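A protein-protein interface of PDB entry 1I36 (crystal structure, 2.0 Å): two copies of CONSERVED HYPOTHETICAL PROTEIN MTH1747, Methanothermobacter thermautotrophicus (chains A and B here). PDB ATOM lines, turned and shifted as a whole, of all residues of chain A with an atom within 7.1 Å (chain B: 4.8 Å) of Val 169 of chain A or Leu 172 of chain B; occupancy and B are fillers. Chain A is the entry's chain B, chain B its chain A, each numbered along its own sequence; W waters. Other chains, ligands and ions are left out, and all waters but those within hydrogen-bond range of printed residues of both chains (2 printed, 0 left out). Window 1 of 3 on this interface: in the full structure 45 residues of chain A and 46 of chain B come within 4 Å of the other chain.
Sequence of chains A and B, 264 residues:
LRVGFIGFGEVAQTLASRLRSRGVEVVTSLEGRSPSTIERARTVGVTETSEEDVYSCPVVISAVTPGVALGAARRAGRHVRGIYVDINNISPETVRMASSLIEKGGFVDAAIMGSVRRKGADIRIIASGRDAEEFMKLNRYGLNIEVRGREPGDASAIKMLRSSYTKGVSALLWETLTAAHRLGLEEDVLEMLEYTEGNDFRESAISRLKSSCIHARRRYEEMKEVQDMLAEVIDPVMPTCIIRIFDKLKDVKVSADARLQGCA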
ATOM      1  N   SER A 163     -28.701   0.095  35.789  1.00  0.00           N
ATOM      2  CA  SER A 163     -30.075  -0.208  35.417  1.00  0.00           C
ATOM      3  C   SER A 163     -30.436   0.459  34.077  1.00  0.00           C
ATOM      4  O   SER A 163     -31.172  -0.104  33.276  1.00  0.00           O
ATOM      5  CB  SER A 163     -31.009   0.262  36.518  1.00  0.00           C
ATOM      6  OG  SER A 163     -32.363   0.152  36.115  1.00  0.00           O
ATOM      7  N   SER A 164     -29.902   1.654  33.835  1.00  0.00           N
ATOM      8  CA  SER A 164     -30.144   2.373  32.595  1.00  0.00           C
ATOM      9  C   SER A 164     -29.601   1.554  31.414  1.00  0.00           C
ATOM     10  O   SER A 164     -30.255   1.393  30.377  1.00  0.00           O
ATOM     11  CB  SER A 164     -29.420   3.706  32.637  1.00  0.00           C
ATOM     12  OG  SER A 164     -29.564   4.392  31.418  1.00  0.00           O
ATOM     13  N   TYR A 165     -28.382   1.069  31.583  1.00  0.00           N
ATOM     14  CA  TYR A 165     -27.736   0.271  30.550  1.00  0.00           C
ATOM     15  C   TYR A 165     -28.507  -1.017  30.307  1.00  0.00           C
ATOM     16  O   TYR A 165     -28.841  -1.334  29.155  1.00  0.00           O
ATOM     17  CB  TYR A 165     -26.290  -0.031  30.943  1.00  0.00           C
ATOM     18  CG  TYR A 165     -25.607  -0.993  30.009  1.00  0.00           C
ATOM     19  CD1 TYR A 165     -24.993  -0.536  28.842  1.00  0.00           C
ATOM     20  CD2 TYR A 165     -25.589  -2.363  30.277  1.00  0.00           C
ATOM     21  CE1 TYR A 165     -24.376  -1.422  27.955  1.00  0.00           C
ATOM     22  CE2 TYR A 165     -24.975  -3.261  29.391  1.00  0.00           C
ATOM     23  CZ  TYR A 165     -24.377  -2.770  28.233  1.00  0.00           C
ATOM     24  OH  TYR A 165     -23.797  -3.644  27.344  1.00  0.00           O
ATOM     25  N   THR A 166     -28.799  -1.758  31.374  1.00  0.00           N
ATOM     26  CA  THR A 166     -29.506  -3.019  31.236  1.00  0.00           C
ATOM     27  C   THR A 166     -30.910  -2.855  30.618  1.00  0.00           C
ATOM     28  O   THR A 166     -31.318  -3.706  29.805  1.00  0.00           O
ATOM     29  CB  THR A 166     -29.550  -3.799  32.566  1.00  0.00           C
ATOM     30  OG1 THR A 166     -30.295  -3.059  33.537  1.00  0.00           O
ATOM     31  CG2 THR A 166     -28.162  -4.012  33.085  1.00  0.00           C
ATOM     32  N   LYS A 167     -31.617  -1.756  30.932  1.00  0.00           N
ATOM     33  CA  LYS A 167     -32.940  -1.522  30.339  1.00  0.00           C
ATOM     34  C   LYS A 167     -32.803  -1.194  28.850  1.00  0.00           C
ATOM     35  O   LYS A 167     -33.620  -1.624  28.034  1.00  0.00           O
ATOM     36  CB  LYS A 167     -33.700  -0.394  31.039  1.00  0.00           C
ATOM     37  CG  LYS A 167     -34.317  -0.809  32.375  1.00  0.00           C
ATOM     38  CD  LYS A 167     -35.331   0.231  32.843  1.00  0.00           C
ATOM     39  CE  LYS A 167     -34.643   1.464  33.385  1.00  0.00           C
ATOM     40  NZ  LYS A 167     -34.015   1.141  34.697  1.00  0.00           N
ATOM     41  N   GLY A 168     -31.785  -0.416  28.510  1.00  0.00           N
ATOM     42  CA  GLY A 168     -31.537  -0.071  27.124  1.00  0.00           C
ATOM     43  C   GLY A 168     -31.226  -1.331  26.315  1.00  0.00           C
ATOM     44  O   GLY A 168     -31.755  -1.506  25.228  1.00  0.00           O
ATOM     45  N   VAL A 169     -30.401  -2.220  26.862  1.00  0.00           N
ATOM     46  CA  VAL A 169     -30.039  -3.455  26.167  1.00  0.00           C
ATOM     47  C   VAL A 169     -31.298  -4.314  25.960  1.00  0.00           C
ATOM     48  O   VAL A 169     -31.476  -4.928  24.903  1.00  0.00           O
ATOM     49  CB  VAL A 169     -28.944  -4.230  26.953  1.00  0.00           C
ATOM     50  CG1 VAL A 169     -28.769  -5.666  26.418  1.00  0.00           C
ATOM     51  CG2 VAL A 169     -27.645  -3.479  26.874  1.00  0.00           C
ATOM     52  N   SER A 170     -32.162  -4.371  26.970  1.00  0.00           N
ATOM     53  CA  SER A 170     -33.392  -5.140  26.859  1.00  0.00           C
ATOM     54  C   SER A 170     -34.270  -4.615  25.730  1.00  0.00           C
ATOM     55  O   SER A 170     -34.816  -5.413  24.971  1.00  0.00           O
ATOM     56  CB  SER A 170     -34.188  -5.099  28.159  1.00  0.00           C
ATOM     57  OG  SER A 170     -33.614  -5.969  29.108  1.00  0.00           O
ATOM     58  N   ALA A 171     -34.370  -3.289  25.607  1.00  0.00           N
ATOM     59  CA  ALA A 171     -35.166  -2.662  24.556  1.00  0.00           C
ATOM     60  C   ALA A 171     -34.574  -2.968  23.171  1.00  0.00           C
ATOM     61  O   ALA A 171     -35.306  -3.285  22.222  1.00  0.00           O
ATOM     62  CB  ALA A 171     -35.251  -1.155  24.772  1.00  0.00           C
ATOM     63  N   LEU A 172     -33.253  -2.885  23.076  1.00  0.00           N
ATOM     64  CA  LEU A 172     -32.531  -3.168  21.839  1.00  0.00           C
ATOM     65  C   LEU A 172     -32.752  -4.636  21.415  1.00  0.00           C
ATOM     66  O   LEU A 172     -33.008  -4.936  20.224  1.00  0.00           O
ATOM     67  CB  LEU A 172     -31.048  -2.892  22.052  1.00  0.00           C
ATOM     68  CG  LEU A 172     -30.110  -3.172  20.875  1.00  0.00           C
ATOM     69  CD1 LEU A 172     -30.446  -2.228  19.711  1.00  0.00           C
ATOM     70  CD2 LEU A 172     -28.679  -2.985  21.326  1.00  0.00           C
ATOM     71  N   LEU A 173     -32.662  -5.544  22.386  1.00  0.00           N
ATOM     72  CA  LEU A 173     -32.855  -6.969  22.130  1.00  0.00           C
ATOM     73  C   LEU A 173     -34.283  -7.205  21.609  1.00  0.00           C
ATOM     74  O   LEU A 173     -34.473  -7.938  20.647  1.00  0.00           O
ATOM     75  CB  LEU A 173     -32.597  -7.807  23.389  1.00  0.00           C
ATOM     76  CG  LEU A 173     -32.693  -9.329  23.168  1.00  0.00           C
ATOM     77  CD1 LEU A 173     -31.591  -9.815  22.236  1.00  0.00           C
ATOM     78  CD2 LEU A 173     -32.581 -10.073  24.512  1.00  0.00           C
ATOM     79  N   TRP A 174     -35.274  -6.601  22.259  1.00  0.00           N
ATOM     80  CA  TRP A 174     -36.650  -6.724  21.803  1.00  0.00           C
ATOM     81  C   TRP A 174     -36.836  -6.270  20.332  1.00  0.00           C
ATOM     82  O   TRP A 174     -37.409  -7.001  19.512  1.00  0.00           O
ATOM     83  CB  TRP A 174     -37.590  -5.909  22.686  1.00  0.00           C
ATOM     84  CG  TRP A 174     -39.030  -6.083  22.259  1.00  0.00           C
ATOM     85  CD1 TRP A 174     -39.858  -7.121  22.580  1.00  0.00           C
ATOM     86  CD2 TRP A 174     -39.776  -5.230  21.384  1.00  0.00           C
ATOM     87  NE1 TRP A 174     -41.068  -6.965  21.955  1.00  0.00           N
ATOM     88  CE2 TRP A 174     -41.046  -5.809  21.219  1.00  0.00           C
ATOM     89  CE3 TRP A 174     -39.490  -4.033  20.718  1.00  0.00           C
ATOM     90  CZ2 TRP A 174     -42.030  -5.237  20.410  1.00  0.00           C
ATOM     91  CZ3 TRP A 174     -40.467  -3.460  19.912  1.00  0.00           C
ATOM     92  CH2 TRP A 174     -41.720  -4.062  19.769  1.00  0.00           C
ATOM     93  N   GLU A 175     -36.350  -5.071  19.995  1.00  0.00           N
ATOM     94  CA  GLU A 175     -36.514  -4.583  18.637  1.00  0.00           C
ATOM     95  C   GLU A 175     -35.800  -5.516  17.653  1.00  0.00           C
ATOM     96  O   GLU A 175     -36.393  -5.941  16.670  1.00  0.00           O
ATOM     97  CB  GLU A 175     -36.031  -3.145  18.494  1.00  0.00           C
ATOM     98  CG  GLU A 175     -36.188  -2.631  17.085  1.00  0.00           C
ATOM     99  CD  GLU A 175     -36.234  -1.146  17.007  1.00  0.00           C
ATOM    100  OE1 GLU A 175     -35.164  -0.506  17.004  1.00  0.00           O
ATOM    101  OE2 GLU A 175     -37.350  -0.614  16.889  1.00  0.00           O
ATOM    102  N   THR A 176     -34.585  -5.931  17.995  1.00  0.00           N
ATOM    103  CA  THR A 176     -33.808  -6.847  17.172  1.00  0.00           C
ATOM    104  C   THR A 176     -34.561  -8.166  16.951  1.00  0.00           C
ATOM    105  O   THR A 176     -34.681  -8.627  15.813  1.00  0.00           O
ATOM    106  CB  THR A 176     -32.450  -7.150  17.814  1.00  0.00           C
ATOM    107  OG1 THR A 176     -31.732  -5.926  17.935  1.00  0.00           O
ATOM    108  CG2 THR A 176     -31.628  -8.097  16.927  1.00  0.00           C
ATOM    109  N   GLU A 197     -21.474 -12.462  22.654  1.00  0.00           N
ATOM    110  CA  GLU A 197     -22.019 -11.844  23.859  1.00  0.00           C
ATOM    111  C   GLU A 197     -21.846 -12.727  25.098  1.00  0.00           C
ATOM    112  O   GLU A 197     -22.231 -12.337  26.208  1.00  0.00           O
ATOM    113  CB  GLU A 197     -23.500 -11.505  23.668  1.00  0.00           C
ATOM    114  CG  GLU A 197     -23.825 -10.658  22.430  1.00  0.00           C
ATOM    115  CD  GLU A 197     -23.084  -9.335  22.393  1.00  0.00           C
ATOM    116  OE1 GLU A 197     -23.295  -8.494  23.301  1.00  0.00           O
ATOM    117  OE2 GLU A 197     -22.294  -9.133  21.451  1.00  0.00           O
ATOM    118  N   PHE A 201     -25.488 -16.198  27.680  1.00  0.00           N
ATOM    119  CA  PHE A 201     -26.213 -15.113  27.031  1.00  0.00           C
ATOM    120  C   PHE A 201     -27.709 -15.334  26.837  1.00  0.00           C
ATOM    121  O   PHE A 201     -28.524 -14.672  27.480  1.00  0.00           O
ATOM    122  CB  PHE A 201     -25.576 -14.788  25.675  1.00  0.00           C
ATOM    123  CG  PHE A 201     -26.334 -13.758  24.880  1.00  0.00           C
ATOM    124  CD1 PHE A 201     -26.321 -12.419  25.262  1.00  0.00           C
ATOM    125  CD2 PHE A 201     -27.090 -14.130  23.772  1.00  0.00           C
ATOM    126  CE1 PHE A 201     -27.054 -11.466  24.554  1.00  0.00           C
ATOM    127  CE2 PHE A 201     -27.825 -13.187  23.062  1.00  0.00           C
ATOM    128  CZ  PHE A 201     -27.808 -11.855  23.451  1.00  0.00           C
ATOM    129  N   ARG A 208     -34.736 -11.442  30.563  1.00  0.00           N
ATOM    130  CA  ARG A 208     -34.922  -9.998  30.569  1.00  0.00           C
ATOM    131  C   ARG A 208     -36.011  -9.566  29.583  1.00  0.00           C
ATOM    132  O   ARG A 208     -36.713  -8.579  29.818  1.00  0.00           O
ATOM    133  CB  ARG A 208     -33.607  -9.271  30.274  1.00  0.00           C
ATOM    134  CG  ARG A 208     -33.198  -9.202  28.797  1.00  0.00           C
ATOM    135  CD  ARG A 208     -32.018  -8.276  28.633  1.00  0.00           C
ATOM    136  NE  ARG A 208     -31.278  -8.544  27.409  1.00  0.00           N
ATOM    137  CZ  ARG A 208     -29.952  -8.622  27.344  1.00  0.00           C
ATOM    138  NH1 ARG A 208     -29.229  -8.451  28.448  1.00  0.00           N
ATOM    139  NH2 ARG A 208     -29.345  -8.864  26.177  1.00  0.00           N
ATOM    140  N   SER A 212     -39.151  -7.305  30.889  1.00  0.00           N
ATOM    141  CA  SER A 212     -39.265  -5.969  30.290  1.00  0.00           C
ATOM    142  C   SER A 212     -40.708  -5.726  29.842  1.00  0.00           C
ATOM    143  O   SER A 212     -41.196  -4.589  29.894  1.00  0.00           O
ATOM    144  CB  SER A 212     -38.344  -5.821  29.063  1.00  0.00           C
ATOM    145  OG  SER A 212     -36.972  -5.824  29.425  1.00  0.00           O
ATOM    146  N   MET A 238     -30.029   8.302  24.177  1.00  0.00           N
ATOM    147  CA  MET A 238     -30.710   7.009  24.191  1.00  0.00           C
ATOM    148  C   MET A 238     -32.049   6.834  24.897  1.00  0.00           C
ATOM    149  O   MET A 238     -32.928   6.121  24.388  1.00  0.00           O
ATOM    150  CB  MET A 238     -29.753   5.898  24.650  1.00  0.00           C
ATOM    151  CG  MET A 238     -28.476   5.753  23.818  1.00  0.00           C
ATOM    152  SD  MET A 238     -28.841   5.482  22.061  1.00  0.00           S
ATOM    153  CE  MET A 238     -29.943   4.130  22.171  1.00  0.00           C
ATOM    154  N   PRO A 239     -32.240   7.472  26.077  1.00  0.00           N
ATOM    155  CA  PRO A 239     -33.521   7.300  26.782  1.00  0.00           C
ATOM    156  C   PRO A 239     -34.783   7.529  25.944  1.00  0.00           C
ATOM    157  O   PRO A 239     -35.789   6.814  26.113  1.00  0.00           O
ATOM    158  CB  PRO A 239     -33.422   8.308  27.925  1.00  0.00           C
ATOM    159  CG  PRO A 239     -31.943   8.312  28.241  1.00  0.00           C
ATOM    160  CD  PRO A 239     -31.353   8.380  26.826  1.00  0.00           C
ATOM    161  N   ILE A 242     -35.516   4.361  23.905  1.00  0.00           N
ATOM    162  CA  ILE A 242     -35.812   3.265  24.824  1.00  0.00           C
ATOM    163  C   ILE A 242     -37.234   3.380  25.346  1.00  0.00           C
ATOM    164  O   ILE A 242     -37.975   2.393  25.403  1.00  0.00           O
ATOM    165  CB  ILE A 242     -34.800   3.245  26.019  1.00  0.00           C
ATOM    166  CG1 ILE A 242     -33.378   2.977  25.493  1.00  0.00           C
ATOM    167  CG2 ILE A 242     -35.167   2.114  26.987  1.00  0.00           C
ATOM    168  CD1 ILE A 242     -32.279   3.340  26.500  1.00  0.00           C
ATOM    169  N   TYR B 165     -27.591  -5.115  16.698  1.00  0.00           N
ATOM    170  CA  TYR B 165     -27.537  -5.315  18.152  1.00  0.00           C
ATOM    171  C   TYR B 165     -26.184  -4.899  18.734  1.00  0.00           C
ATOM    172  O   TYR B 165     -26.117  -4.042  19.638  1.00  0.00           O
ATOM    173  CB  TYR B 165     -27.840  -6.778  18.510  1.00  0.00           C
ATOM    174  CG  TYR B 165     -27.794  -7.048  20.000  1.00  0.00           C
ATOM    175  CD1 TYR B 165     -26.641  -7.526  20.601  1.00  0.00           C
ATOM    176  CD2 TYR B 165     -28.907  -6.807  20.803  1.00  0.00           C
ATOM    177  CE1 TYR B 165     -26.587  -7.769  21.975  1.00  0.00           C
ATOM    178  CE2 TYR B 165     -28.870  -7.045  22.191  1.00  0.00           C
ATOM    179  CZ  TYR B 165     -27.712  -7.522  22.762  1.00  0.00           C
ATOM    180  OH  TYR B 165     -27.638  -7.753  24.122  1.00  0.00           O
ATOM    181  N   GLY B 168     -25.690  -1.181  18.663  1.00  0.00           N
ATOM    182  CA  GLY B 168     -26.578  -0.522  19.609  1.00  0.00           C
ATOM    183  C   GLY B 168     -26.011  -0.587  21.036  1.00  0.00           C
ATOM    184  O   GLY B 168     -26.078   0.395  21.752  1.00  0.00           O
ATOM    185  N   VAL B 169     -25.501  -1.751  21.441  1.00  0.00           N
ATOM    186  CA  VAL B 169     -24.897  -1.962  22.764  1.00  0.00           C
ATOM    187  C   VAL B 169     -23.677  -1.044  22.946  1.00  0.00           C
ATOM    188  O   VAL B 169     -23.449  -0.505  24.042  1.00  0.00           O
ATOM    189  CB  VAL B 169     -24.478  -3.448  22.941  1.00  0.00           C
ATOM    190  CG1 VAL B 169     -23.610  -3.639  24.193  1.00  0.00           C
ATOM    191  CG2 VAL B 169     -25.730  -4.323  23.021  1.00  0.00           C
ATOM    192  N   SER B 170     -22.873  -0.890  21.892  1.00  0.00           N
ATOM    193  CA  SER B 170     -21.700   0.006  21.936  1.00  0.00           C
ATOM    194  C   SER B 170     -22.133   1.437  22.218  1.00  0.00           C
ATOM    195  O   SER B 170     -21.475   2.164  22.981  1.00  0.00           O
ATOM    196  CB  SER B 170     -20.943  -0.002  20.596  1.00  0.00           C
ATOM    197  OG  SER B 170     -20.253  -1.230  20.466  1.00  0.00           O
ATOM    198  N   ALA B 171     -23.216   1.866  21.579  1.00  0.00           N
ATOM    199  CA  ALA B 171     -23.714   3.215  21.799  1.00  0.00           C
ATOM    200  C   ALA B 171     -24.282   3.379  23.222  1.00  0.00           C
ATOM    201  O   ALA B 171     -24.134   4.445  23.836  1.00  0.00           O
ATOM    202  CB  ALA B 171     -24.783   3.548  20.784  1.00  0.00           C
ATOM    203  N   LEU B 172     -25.010   2.364  23.686  1.00  0.00           N
ATOM    204  CA  LEU B 172     -25.618   2.389  25.022  1.00  0.00           C
ATOM    205  C   LEU B 172     -24.508   2.419  26.073  1.00  0.00           C
ATOM    206  O   LEU B 172     -24.572   3.180  27.054  1.00  0.00           O
ATOM    207  CB  LEU B 172     -26.507   1.161  25.246  1.00  0.00           C
ATOM    208  CG  LEU B 172     -27.809   1.078  24.444  1.00  0.00           C
ATOM    209  CD1 LEU B 172     -28.375  -0.352  24.501  1.00  0.00           C
ATOM    210  CD2 LEU B 172     -28.865   2.085  24.977  1.00  0.00           C
ATOM    211  N   LEU B 173     -23.470   1.631  25.832  1.00  0.00           N
ATOM    212  CA  LEU B 173     -22.340   1.576  26.749  1.00  0.00           C
ATOM    213  C   LEU B 173     -21.659   2.929  26.824  1.00  0.00           C
ATOM    214  O   LEU B 173     -21.400   3.446  27.917  1.00  0.00           O
ATOM    215  CB  LEU B 173     -21.328   0.553  26.299  1.00  0.00           C
ATOM    216  CG  LEU B 173     -20.171   0.419  27.285  1.00  0.00           C
ATOM    217  CD1 LEU B 173     -20.671  -0.282  28.566  1.00  0.00           C
ATOM    218  CD2 LEU B 173     -19.057  -0.388  26.641  1.00  0.00           C
ATOM    219  N   TRP B 174     -21.362   3.494  25.659  1.00  0.00           N
ATOM    220  CA  TRP B 174     -20.709   4.792  25.586  1.00  0.00           C
ATOM    221  C   TRP B 174     -21.471   5.882  26.323  1.00  0.00           C
ATOM    222  O   TRP B 174     -20.884   6.631  27.103  1.00  0.00           O
ATOM    223  CB  TRP B 174     -20.494   5.225  24.130  1.00  0.00           C
ATOM    224  CG  TRP B 174     -19.766   6.543  24.049  1.00  0.00           C
ATOM    225  CD1 TRP B 174     -18.412   6.744  24.059  1.00  0.00           C
ATOM    226  CD2 TRP B 174     -20.361   7.830  23.991  1.00  0.00           C
ATOM    227  NE1 TRP B 174     -18.137   8.094  24.007  1.00  0.00           N
ATOM    228  CE2 TRP B 174     -19.317   8.778  23.966  1.00  0.00           C
ATOM    229  CE3 TRP B 174     -21.678   8.282  23.947  1.00  0.00           C
ATOM    230  CZ2 TRP B 174     -19.554  10.137  23.904  1.00  0.00           C
ATOM    231  CZ3 TRP B 174     -21.911   9.639  23.885  1.00  0.00           C
ATOM    232  CH2 TRP B 174     -20.862  10.546  23.863  1.00  0.00           C
ATOM    233  N   GLU B 175     -22.768   6.002  26.069  1.00  0.00           N
ATOM    234  CA  GLU B 175     -23.534   7.027  26.746  1.00  0.00           C
ATOM    235  C   GLU B 175     -23.568   6.803  28.270  1.00  0.00           C
ATOM    236  O   GLU B 175     -23.403   7.758  29.045  1.00  0.00           O
ATOM    237  CB  GLU B 175     -24.947   7.139  26.180  1.00  0.00           C
ATOM    238  CG  GLU B 175     -25.809   8.140  26.951  1.00  0.00           C
ATOM    239  CD  GLU B 175     -27.007   8.629  26.185  1.00  0.00           C
ATOM    240  OE1 GLU B 175     -28.081   8.007  26.269  1.00  0.00           O
ATOM    241  OE2 GLU B 175     -26.882   9.669  25.510  1.00  0.00           O
ATOM    242  N   THR B 176     -23.778   5.560  28.690  1.00  0.00           N
ATOM    243  CA  THR B 176     -23.818   5.221  30.117  1.00  0.00           C
ATOM    244  C   THR B 176     -22.487   5.561  30.807  1.00  0.00           C
ATOM    245  O   THR B 176     -22.483   6.189  31.872  1.00  0.00           O
ATOM    246  CB  THR B 176     -24.134   3.731  30.329  1.00  0.00           C
ATOM    247  OG1 THR B 176     -25.464   3.481  29.893  1.00  0.00           O
ATOM    248  CG2 THR B 176     -24.033   3.332  31.815  1.00  0.00           C
ATOM    249  N   MET B 238     -34.907   2.303  17.658  1.00  0.00           N
ATOM    250  CA  MET B 238     -33.566   2.468  18.217  1.00  0.00           C
ATOM    251  C   MET B 238     -32.447   3.040  17.325  1.00  0.00           C
ATOM    252  O   MET B 238     -31.628   3.840  17.791  1.00  0.00           O
ATOM    253  CB  MET B 238     -33.109   1.151  18.877  1.00  0.00           C
ATOM    254  CG  MET B 238     -34.001   0.641  20.010  1.00  0.00           C
ATOM    255  SD  MET B 238     -33.907   1.706  21.493  1.00  0.00           S
ATOM    256  CE  MET B 238     -32.345   1.208  22.149  1.00  0.00           C
HETATM  257  O   HOH W   1     -27.044   5.247  31.054  1.00  0.00           O
HETATM  258  O   HOH W   2     -25.206  -7.802  25.269  1.00  0.00           O
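The backbone NH (N) of Met 238 of chain A lies within hydrogen-bond range of the side-chain carboxylate (OE1) of Glu 175 of chain B. The side-chain hydroxyl (OH) of Tyr 165 of chain B sits at hydrogen-bond distance from the guanidinium group (NH2) of Arg 208 of chain A (2.9 Å). OE1 of Glu 175 of chain A lies within hydrogen-bond range of N of Met 238 of chain B (2.9 Å).
The backbone carbonyl oxygen (O) of Arg 208 of chain A is in hydrogen-bond range of the side-chain hydroxyl (OG) of Ser 212 of chain A (2.8 Å). O of Leu 172 of chain B is in hydrogen-bond range of OG1 of Thr 176 of chain B, 3.0 Å away. The backbone carbonyl oxygen (O) of Leu 172 of chain A is in hydrogen-bond range of the side-chain hydroxyl (OG1) of Thr 176 of chain A.
Among the printed residues, merely in contact across the chains: Tyr 165 of chain A with Val 169 of chain B (3.2 Å), Tyr 165 of chain A with Leu 173 of chain B (3.8 Å), Tyr 165 of chain A with Thr 176 of chain B (3.8 Å), Gly 168 of chain A with Leu 172 of chain B (3.5 Å), Val 169 of chain A with Tyr 165 of chain B (3.3 Å), Val 169 of chain A with Leu 172 of chain B (3.6 Å), Leu 172 of chain A with Tyr 165 of chain B (3.2 Å), Leu 172 of chain A with Gly 168 of chain B (3.6 Å), Leu 172 of chain A with Val 169 of chain B (3.4 Å), Leu 173 of chain A with Tyr 165 of chain B (3.9 Å), Glu 197 of chain A with Tyr 165 of chain B (3.6 Å), Phe 201 of chain A with Tyr 165 of chain B (3.8 Å), Met 238 of chain A with Leu 172 of chain B (3.6 Å), Met 238 of chain A with Met 238 of chain B (3.8 Å), Pro 239 of chain A with Glu 175 of chain B (3.3 Å), Ile 242 of chain A with Leu 172 of chain B (3.9 Å) and Ile 242 of chain A with Met 238 of chain B (3.9 Å).
Of chain A, only Gly 168, Val 169, Met 238 and Ile 242 come within 4 Å of Leu 172 of chain B. Printed residues of chain B within 4 Å of Phe 201 of chain A: Tyr 165 (3.8 Å). Of the printed residues of chain B, Met 238 of chain A touches Leu 172 (3.6 Å), Glu 175 (2.9 Å) and Met 238 (3.8 Å). Of the printed residues of chain A, Val 169 of chain B touches Tyr 165 and Leu 172. Printed residues of chain B within 4 Å of Glu 175 of chain A: Met 238. Of the printed residues of chain B, Leu 173 of chain A touches Tyr 165 (3.9 Å). Thr 176 of chain A touches none of the printed residues of chain B. Ser 212 of chain A touches none of the printed residues of chain B. The nearest residue of chain A that does not touch Leu 172 of chain B is Tyr 165 of chain A (4.1 Å).
Hydrophobic or aromatic side chains of chain A within 4 Å of the printed part of chain B: Tyr 165, Val 169, Leu 172, Leu 173, Phe 201, Met 238, Pro 239 and Ile 242. Of the 11 printed residues of chain B, 8 touch a printed residue of chain A. Among the printed residues, 20 pairs touch across the chains. Among the printed residues, no Asp or Glu carboxylate lies within 4 Å of a Lys or Arg side-chain nitrogen of the other chain.
Tyr 165 of chain A touches Val 169 of chain B, and with the chains exchanged Val 169 of chain A touches Tyr 165 of chain B. Tyr 165 of chain A touches Leu 173 of chain B, and with the chains exchanged Leu 173 of chain A touches Tyr 165 of chain B. Tyr 165 of chain A touches Thr 176 of chain B, but with the chains exchanged Thr 176 of chain A does not touch Tyr 165 of chain B (4.03 Å). Leu 172 of chain A touches Tyr 165 of chain B, but with the chains exchanged Tyr 165 of chain A does not touch Leu 172 of chain B (4.1 Å). 11 positions are printed for both chains.
Water W1 lies within hydrogen-bond range of the side-chain hydroxyl (OG1) of Thr 176 of chain B and the side-chain hydroxyl (OG) of Ser 164 of chain A. Water W2 lies within hydrogen-bond range of the side-chain hydroxyl (OH) of Tyr 165 of chain B (2.7 Å) and the side-chain carboxylate (OE1) of Glu 197 of chain A (2.8 Å).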
